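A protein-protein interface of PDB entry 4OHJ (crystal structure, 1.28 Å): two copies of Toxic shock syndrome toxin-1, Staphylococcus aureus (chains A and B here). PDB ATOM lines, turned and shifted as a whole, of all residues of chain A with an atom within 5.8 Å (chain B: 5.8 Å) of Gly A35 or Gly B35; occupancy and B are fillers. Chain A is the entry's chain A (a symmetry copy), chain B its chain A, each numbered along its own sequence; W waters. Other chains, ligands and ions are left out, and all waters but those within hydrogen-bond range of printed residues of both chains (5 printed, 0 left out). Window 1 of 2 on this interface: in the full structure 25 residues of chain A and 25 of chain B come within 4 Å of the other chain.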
ATOM      1  N   ASP A  30      10.052  -6.706  10.167  1.00  0.00           N
ATOM      2  CA  ASP A  30       9.279  -5.570   9.681  1.00  0.00           C
ATOM      3  C   ASP A  30       8.222  -5.136  10.707  1.00  0.00           C
ATOM      4  O   ASP A  30       8.094  -3.961  11.020  1.00  0.00           O
ATOM      5  CB  ASP A  30       8.503  -5.915   8.389  1.00  0.00           C
ATOM      6  CG  ASP A  30       9.313  -5.884   7.150  1.00  0.00           C
ATOM      7  OD1 ASP A  30      10.442  -5.347   7.144  1.00  0.00           O
ATOM      8  OD2 ASP A  30       8.724  -6.300   6.111  1.00  0.00           O
ATOM      9  N   TRP A  31       7.457  -6.081  11.223  1.00  0.00           N
ATOM     10  CA  TRP A  31       6.386  -5.758  12.153  1.00  0.00           C
ATOM     11  C   TRP A  31       6.925  -5.058  13.384  1.00  0.00           C
ATOM     12  O   TRP A  31       6.411  -4.041  13.803  1.00  0.00           O
ATOM     13  CB  TRP A  31       5.622  -7.029  12.532  1.00  0.00           C
ATOM     14  CG  TRP A  31       4.508  -6.811  13.523  1.00  0.00           C
ATOM     15  CD1 TRP A  31       4.550  -7.015  14.860  1.00  0.00           C
ATOM     16  CD2 TRP A  31       3.191  -6.316  13.240  1.00  0.00           C
ATOM     17  NE1 TRP A  31       3.353  -6.733  15.431  1.00  0.00           N
ATOM     18  CE2 TRP A  31       2.498  -6.286  14.460  1.00  0.00           C
ATOM     19  CE3 TRP A  31       2.539  -5.883  12.088  1.00  0.00           C
ATOM     20  CZ2 TRP A  31       1.187  -5.868  14.558  1.00  0.00           C
ATOM     21  CZ3 TRP A  31       1.229  -5.458  12.200  1.00  0.00           C
ATOM     22  CH2 TRP A  31       0.577  -5.460  13.417  1.00  0.00           C
ATOM     23  N   TYR A  32       7.987  -5.608  13.952  1.00  0.00           N
ATOM     24  CA  TYR A  32       8.518  -5.061  15.204  1.00  0.00           C
ATOM     25  C   TYR A  32       9.403  -3.826  15.046  1.00  0.00           C
ATOM     26  O   TYR A  32       9.795  -3.221  16.043  1.00  0.00           O
ATOM     27  CB  TYR A  32       9.136  -6.155  16.074  1.00  0.00           C
ATOM     28  CG  TYR A  32       8.078  -7.099  16.589  1.00  0.00           C
ATOM     29  CD1 TYR A  32       7.218  -6.694  17.613  1.00  0.00           C
ATOM     30  CD2 TYR A  32       7.902  -8.370  16.065  1.00  0.00           C
ATOM     31  CE1 TYR A  32       6.270  -7.531  18.124  1.00  0.00           C
ATOM     32  CE2 TYR A  32       6.909  -9.210  16.532  1.00  0.00           C
ATOM     33  CZ  TYR A  32       6.100  -8.804  17.576  1.00  0.00           C
ATOM     34  OH  TYR A  32       5.140  -9.627  18.111  1.00  0.00           O
ATOM     35  N   SER A  33       9.679  -3.408  13.826  1.00  0.00           N
ATOM     36  CA  SER A  33      10.437  -2.184  13.663  1.00  0.00           C
ATOM     37  C   SER A  33       9.607  -1.124  12.887  1.00  0.00           C
ATOM     38  O   SER A  33      10.166  -0.114  12.448  1.00  0.00           O
ATOM     39  CB  SER A  33      11.814  -2.445  13.041  1.00  0.00           C
ATOM     40  OG  SER A  33      11.659  -3.029  11.767  1.00  0.00           O
ATOM     41  N   SER A  34       8.284  -1.327  12.764  1.00  0.00           N
ATOM     42  CA  SER A  34       7.408  -0.407  12.068  1.00  0.00           C
ATOM     43  C   SER A  34       6.727   0.618  12.962  1.00  0.00           C
ATOM     44  O   SER A  34       5.848   1.337  12.522  1.00  0.00           O
ATOM     45  CB  SER A  34       6.399  -1.210  11.253  1.00  0.00           C
ATOM     46  OG  SER A  34       5.555  -1.947  12.102  1.00  0.00           O
ATOM     47  N   GLY A  35       7.169   0.750  14.204  1.00  0.00           N
ATOM     48  CA  GLY A  35       6.598   1.727  15.085  1.00  0.00           C
ATOM     49  C   GLY A  35       5.255   1.345  15.634  1.00  0.00           C
ATOM     50  O   GLY A  35       4.752   0.244  15.428  1.00  0.00           O
ATOM     51  N   SER A  36       4.672   2.261  16.374  1.00  0.00           N
ATOM     52  CA  SER A  36       3.370   2.046  16.979  1.00  0.00           C
ATOM     53  C   SER A  36       2.733   3.404  17.199  1.00  0.00           C
ATOM     54  O   SER A  36       3.401   4.456  17.120  1.00  0.00           O
ATOM     55  CB  SER A  36       3.493   1.298  18.308  1.00  0.00           C
ATOM     56  OG  SER A  36       4.163   2.094  19.275  1.00  0.00           O
ATOM     57  N   ASP A  37       1.434   3.381  17.484  1.00  0.00           N
ATOM     58  CA  ASP A  37       0.691   4.581  17.741  1.00  0.00           C
ATOM     59  C   ASP A  37       0.300   4.704  19.202  1.00  0.00           C
ATOM     60  O   ASP A  37      -0.271   3.789  19.779  1.00  0.00           O
ATOM     61  CB  ASP A  37      -0.583   4.532  16.917  1.00  0.00           C
ATOM     62  CG  ASP A  37      -0.303   4.509  15.434  1.00  0.00           C
ATOM     63  OD1 ASP A  37       0.564   5.292  14.983  1.00  0.00           O
ATOM     64  OD2 ASP A  37      -0.890   3.699  14.701  1.00  0.00           O
ATOM     65  N   THR A  85      -0.942   0.997  20.291  1.00  0.00           N
ATOM     66  CA  THR A  85      -1.423   0.032  19.356  1.00  0.00           C
ATOM     67  C   THR A  85      -0.636   0.017  18.063  1.00  0.00           C
ATOM     68  O   THR A  85       0.161   0.888  17.765  1.00  0.00           O
ATOM     69  CB  THR A  85      -2.929   0.335  19.076  1.00  0.00           C
ATOM     70  OG1 THR A  85      -3.526  -0.720  18.328  1.00  0.00           O
ATOM     71  CG2 THR A  85      -3.142   1.642  18.346  1.00  0.00           C
ATOM     72  N   LYS A  86      -0.865  -1.025  17.281  1.00  0.00           N
ATOM     73  CA  LYS A  86      -0.186  -1.229  15.997  1.00  0.00           C
ATOM     74  C   LYS A  86      -1.199  -1.152  14.854  1.00  0.00           C
ATOM     75  O   LYS A  86      -2.319  -1.631  14.999  1.00  0.00           O
ATOM     76  CB  LYS A  86       0.488  -2.628  15.949  1.00  0.00           C
ATOM     77  CG  LYS A  86       1.548  -2.909  17.013  1.00  0.00           C
ATOM     78  CD  LYS A  86       2.905  -2.287  16.730  1.00  0.00           C
ATOM     79  CE  LYS A  86       3.770  -3.107  15.787  1.00  0.00           C
ATOM     80  NZ  LYS A  86       5.118  -2.464  15.592  1.00  0.00           N
ATOM     81  N   PHE A 150       5.061  -5.744  21.985  1.00  0.00           N
ATOM     82  CA  PHE A 150       5.811  -4.987  21.008  1.00  0.00           C
ATOM     83  C   PHE A 150       6.886  -4.125  21.610  1.00  0.00           C
ATOM     84  O   PHE A 150       7.915  -3.921  20.969  1.00  0.00           O
ATOM     85  CB  PHE A 150       4.947  -4.273  19.948  1.00  0.00           C
ATOM     86  CG  PHE A 150       4.117  -3.090  20.425  1.00  0.00           C
ATOM     87  CD1 PHE A 150       4.715  -1.888  20.765  1.00  0.00           C
ATOM     88  CD2 PHE A 150       2.741  -3.135  20.380  1.00  0.00           C
ATOM     89  CE1 PHE A 150       3.944  -0.781  21.112  1.00  0.00           C
ATOM     90  CE2 PHE A 150       1.975  -2.033  20.692  1.00  0.00           C
ATOM     91  CZ  PHE A 150       2.565  -0.871  21.073  1.00  0.00           C
ATOM     92  N   ASP B  30       2.955  10.615  11.554  1.00  0.00           N
ATOM     93  CA  ASP B  30       3.142   9.332  10.890  1.00  0.00           C
ATOM     94  C   ASP B  30       4.633   9.007  10.715  1.00  0.00           C
ATOM     95  O   ASP B  30       5.079   7.912  11.028  1.00  0.00           O
ATOM     96  CB  ASP B  30       2.535   9.326   9.468  1.00  0.00           C
ATOM     97  CG  ASP B  30       1.068   9.130   9.419  1.00  0.00           C
ATOM     98  OD1 ASP B  30       0.449   8.722  10.426  1.00  0.00           O
ATOM     99  OD2 ASP B  30       0.544   9.265   8.276  1.00  0.00           O
ATOM    100  N   TRP B  31       5.401   9.953  10.206  1.00  0.00           N
ATOM    101  CA  TRP B  31       6.812   9.716   9.943  1.00  0.00           C
ATOM    102  C   TRP B  31       7.547   9.337  11.213  1.00  0.00           C
ATOM    103  O   TRP B  31       8.292   8.379  11.245  1.00  0.00           O
ATOM    104  CB  TRP B  31       7.437  10.952   9.291  1.00  0.00           C
ATOM    105  CG  TRP B  31       8.911  10.825   9.008  1.00  0.00           C
ATOM    106  CD1 TRP B  31       9.933  11.298   9.758  1.00  0.00           C
ATOM    107  CD2 TRP B  31       9.517  10.150   7.896  1.00  0.00           C
ATOM    108  NE1 TRP B  31      11.128  11.015   9.183  1.00  0.00           N
ATOM    109  CE2 TRP B  31      10.905  10.296   8.039  1.00  0.00           C
ATOM    110  CE3 TRP B  31       9.028   9.429   6.809  1.00  0.00           C
ATOM    111  CZ2 TRP B  31      11.803   9.773   7.133  1.00  0.00           C
ATOM    112  CZ3 TRP B  31       9.938   8.903   5.912  1.00  0.00           C
ATOM    113  CH2 TRP B  31      11.297   9.084   6.081  1.00  0.00           C
ATOM    114  N   TYR B  32       7.315  10.097  12.272  1.00  0.00           N
ATOM    115  CA  TYR B  32       8.056   9.871  13.516  1.00  0.00           C
ATOM    116  C   TYR B  32       7.532   8.728  14.382  1.00  0.00           C
ATOM    117  O   TYR B  32       8.158   8.381  15.384  1.00  0.00           O
ATOM    118  CB  TYR B  32       8.272  11.176  14.283  1.00  0.00           C
ATOM    119  CG  TYR B  32       9.213  12.091  13.539  1.00  0.00           C
ATOM    120  CD1 TYR B  32      10.583  11.814  13.515  1.00  0.00           C
ATOM    121  CD2 TYR B  32       8.768  13.205  12.845  1.00  0.00           C
ATOM    122  CE1 TYR B  32      11.467  12.636  12.878  1.00  0.00           C
ATOM    123  CE2 TYR B  32       9.644  14.016  12.147  1.00  0.00           C
ATOM    124  CZ  TYR B  32      10.999  13.747  12.174  1.00  0.00           C
ATOM    125  OH  TYR B  32      11.911  14.558  11.545  1.00  0.00           O
ATOM    126  N   SER B  33       6.438   8.103  13.996  1.00  0.00           N
ATOM    127  CA  SER B  33       5.983   6.955  14.756  1.00  0.00           C
ATOM    128  C   SER B  33       5.965   5.681  13.868  1.00  0.00           C
ATOM    129  O   SER B  33       5.386   4.667  14.268  1.00  0.00           O
ATOM    130  CB  SER B  33       4.643   7.226  15.451  1.00  0.00           C
ATOM    131  OG  SER B  33       3.658   7.522  14.487  1.00  0.00           O
ATOM    132  N   SER B  34       6.630   5.719  12.700  1.00  0.00           N
ATOM    133  CA  SER B  34       6.688   4.591  11.791  1.00  0.00           C
ATOM    134  C   SER B  34       7.911   3.704  11.961  1.00  0.00           C
ATOM    135  O   SER B  34       8.155   2.824  11.154  1.00  0.00           O
ATOM    136  CB  SER B  34       6.553   5.106  10.361  1.00  0.00           C
ATOM    137  OG  SER B  34       7.656   5.908  10.020  1.00  0.00           O
ATOM    138  N   GLY B  35       8.655   3.871  13.045  1.00  0.00           N
ATOM    139  CA  GLY B  35       9.798   3.039  13.286  1.00  0.00           C
ATOM    140  C   GLY B  35      10.993   3.383  12.447  1.00  0.00           C
ATOM    141  O   GLY B  35      11.013   4.362  11.706  1.00  0.00           O
ATOM    142  N   SER B  36      12.024   2.581  12.586  1.00  0.00           N
ATOM    143  CA  SER B  36      13.257   2.778  11.845  1.00  0.00           C
ATOM    144  C   SER B  36      13.950   1.434  11.735  1.00  0.00           C
ATOM    145  O   SER B  36      13.599   0.462  12.437  1.00  0.00           O
ATOM    146  CB  SER B  36      14.168   3.788  12.547  1.00  0.00           C
ATOM    147  OG  SER B  36      14.626   3.276  13.790  1.00  0.00           O
ATOM    148  N   ASP B  37      14.945   1.381  10.855  1.00  0.00           N
ATOM    149  CA  ASP B  37      15.715   0.187  10.649  1.00  0.00           C
ATOM    150  C   ASP B  37      17.126   0.322  11.190  1.00  0.00           C
ATOM    151  O   ASP B  37      17.831   1.271  10.876  1.00  0.00           O
ATOM    152  CB  ASP B  37      15.807  -0.062   9.155  1.00  0.00           C
ATOM    153  CG  ASP B  37      14.454  -0.310   8.533  1.00  0.00           C
ATOM    154  OD1 ASP B  37      13.661  -1.075   9.127  1.00  0.00           O
ATOM    155  OD2 ASP B  37      14.134   0.270   7.485  1.00  0.00           O
ATOM    156  N   THR B  85      18.351   4.024  10.068  1.00  0.00           N
ATOM    157  CA  THR B  85      17.790   4.726   8.959  1.00  0.00           C
ATOM    158  C   THR B  85      16.289   4.562   8.851  1.00  0.00           C
ATOM    159  O   THR B  85      15.669   3.735   9.494  1.00  0.00           O
ATOM    160  CB  THR B  85      18.491   4.220   7.659  1.00  0.00           C
ATOM    161  OG1 THR B  85      18.139   5.035   6.545  1.00  0.00           O
ATOM    162  CG2 THR B  85      18.168   2.778   7.338  1.00  0.00           C
ATOM    163  N   LYS B  86      15.694   5.395   8.015  1.00  0.00           N
ATOM    164  CA  LYS B  86      14.245   5.404   7.787  1.00  0.00           C
ATOM    165  C   LYS B  86      13.940   4.995   6.346  1.00  0.00           C
ATOM    166  O   LYS B  86      14.671   5.375   5.438  1.00  0.00           O
ATOM    167  CB  LYS B  86      13.662   6.826   8.016  1.00  0.00           C
ATOM    168  CG  LYS B  86      13.855   7.424   9.409  1.00  0.00           C
ATOM    169  CD  LYS B  86      12.888   6.901  10.459  1.00  0.00           C
ATOM    170  CE  LYS B  86      11.538   7.598  10.449  1.00  0.00           C
ATOM    171  NZ  LYS B  86      10.649   7.071  11.545  1.00  0.00           N
ATOM    172  N   PHE B 150      15.451  11.549  14.462  1.00  0.00           N
ATOM    173  CA  PHE B 150      14.304  10.692  14.660  1.00  0.00           C
ATOM    174  C   PHE B 150      14.236  10.085  16.034  1.00  0.00           C
ATOM    175  O   PHE B 150      13.135   9.863  16.533  1.00  0.00           O
ATOM    176  CB  PHE B 150      14.043   9.694  13.513  1.00  0.00           C
ATOM    177  CG  PHE B 150      15.038   8.553  13.360  1.00  0.00           C
ATOM    178  CD1 PHE B 150      15.079   7.512  14.272  1.00  0.00           C
ATOM    179  CD2 PHE B 150      15.813   8.446  12.226  1.00  0.00           C
ATOM    180  CE1 PHE B 150      15.927   6.424  14.076  1.00  0.00           C
ATOM    181  CE2 PHE B 150      16.630   7.357  12.013  1.00  0.00           C
ATOM    182  CZ  PHE B 150      16.704   6.363  12.935  1.00  0.00           C
HETATM  183  O   HOH W   1       6.553   4.543  17.391  1.00  0.00           O
HETATM  184  O   HOH W   2      11.956   0.757  15.124  1.00  0.00           O
HETATM  185  O   HOH W   3      14.226  -3.351  10.553  1.00  0.00           O
HETATM  186  O   HOH W   4       1.133   7.854  15.784  1.00  0.00           O
HETATM  187  O   HOH W   5       5.786   1.774   9.452  1.00  0.00           O
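The side-chain hydroxyl (OG) of Ser B34 sits close to the backbone carbonyl oxygen (O) of Asp B30, at 3.4 Å.
The side-chain hydroxyl of Ser B34 is in hydrogen-bond range of the backbone carbonyl oxygen of Trp B31 (2.8 Å).
The side-chain amino group of Lys B86 lies within hydrogen-bond range of the backbone carbonyl oxygen of Gly B35, at 2.7 Å.
N of Asp B37 lies within hydrogen-bond range of O of Thr B85 (2.8 Å).
O of Asp A30 sits close to OG of Ser A34.
The backbone carbonyl oxygen of Trp A31 sits at hydrogen-bond distance from the side-chain hydroxyl of Ser A34, at 2.8 Å.
Of the printed residues of chain B, Gly A35 touches Ser B33 (3.3 Å), Ser B34 (3.8 Å) and Gly B35 (3.6 Å).
Printed residues of chain A within 4 Å of Gly B35: Ser A33 (3.3 Å), Ser A34 (3.8 Å) and Gly A35 (3.6 Å).
Printed residues of chain B within 4 Å of Ser A36: Ser B33 (3.3 Å).
Of the printed residues of chain B, Asp A37 touches Ser B33 (3.8 Å).
Printed residues of chain B within 4 Å of Ser A34: Ser B33, Ser B34 and Gly B35.
Of the printed residues of chain A, Ser B34 touches Ser A33, Ser A34 and Gly A35.
Trp A31 touches none of the printed residues of chain B.
Thr A85 touches none of the printed residues of chain B.
The nearest printed residue of chain A that does not touch Gly B35 is Ser A36 (5.4 Å).
Among the printed residues, merely in contact across the chains: Ser A33 with Gly B35, Gly A35 with Ser B33, Gly A35 with Gly B35, Ser A34 with Gly B35, Gly A35 with Ser B34, Ser A33 with Ser B34, Ser A34 with Ser B33, Asp A37 with Ser B33 and Ser A33 with Asp B37.
Water W4 lies within hydrogen-bond range of OD1 of Asp A37 (2.7 Å) and OG of Ser B33 (2.9 Å).
Water W3 bridges OD1 of Asp B37 (2.7 Å) and OG of Ser A33 (2.9 Å).
Water W5 bridges O of Ser B34 (3.1 Å) and O of Ser A34 (3.1 Å).
Water W1 lies within hydrogen-bond range of the backbone NH (N) of Ser A36 and the backbone carbonyl oxygen (O) of Ser B33.
Water W2 bridges the backbone NH (N) of Ser B36 (3.1 Å) and the backbone carbonyl oxygen (O) of Ser A33 (3.3 Å).
Ser A33 touches Ser B34, and with the chains exchanged Ser A34 touches Ser B33.
Ser A33 touches Ser B36, and with the chains exchanged Ser A36 touches Ser B33.
Ser A33 touches Asp B37, and with the chains exchanged Asp A37 touches Ser B33.
Ser A34 touches Gly B35, and with the chains exchanged Gly A35 touches Ser B34.
Positions printed for both chains: 30, 31, 32, 33, 34, 35, 36, 37, 85, 86 and 150.
Printed residues of chain A that touch a printed residue of chain B: Ser A33, Ser A34, Gly A35, Ser A36 and Asp A37.
Of the 11 printed residues of chain B, 5 touch a printed residue of chain A.
Along chain B the printed residues that touch a printed residue of chain A span positions 33 to 37.
Among the printed residues, 12 pairs touch across the chains.
Among the printed residues, no Asp or Glu carboxylate lies within 4 Å of a Lys or Arg side-chain nitrogen of the other chain.
The backbone NH (N) of Ser A36 lies within hydrogen-bond range of the backbone carbonyl oxygen (O) of Ser B33, at 3.3 Å.
N of Ser B36 sits at hydrogen-bond distance from O of Ser A33 (3.3 Å).
The backbone carbonyl oxygen of Ser A34 sits close to the backbone carbonyl oxygen of Ser B34 (3.1 Å).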
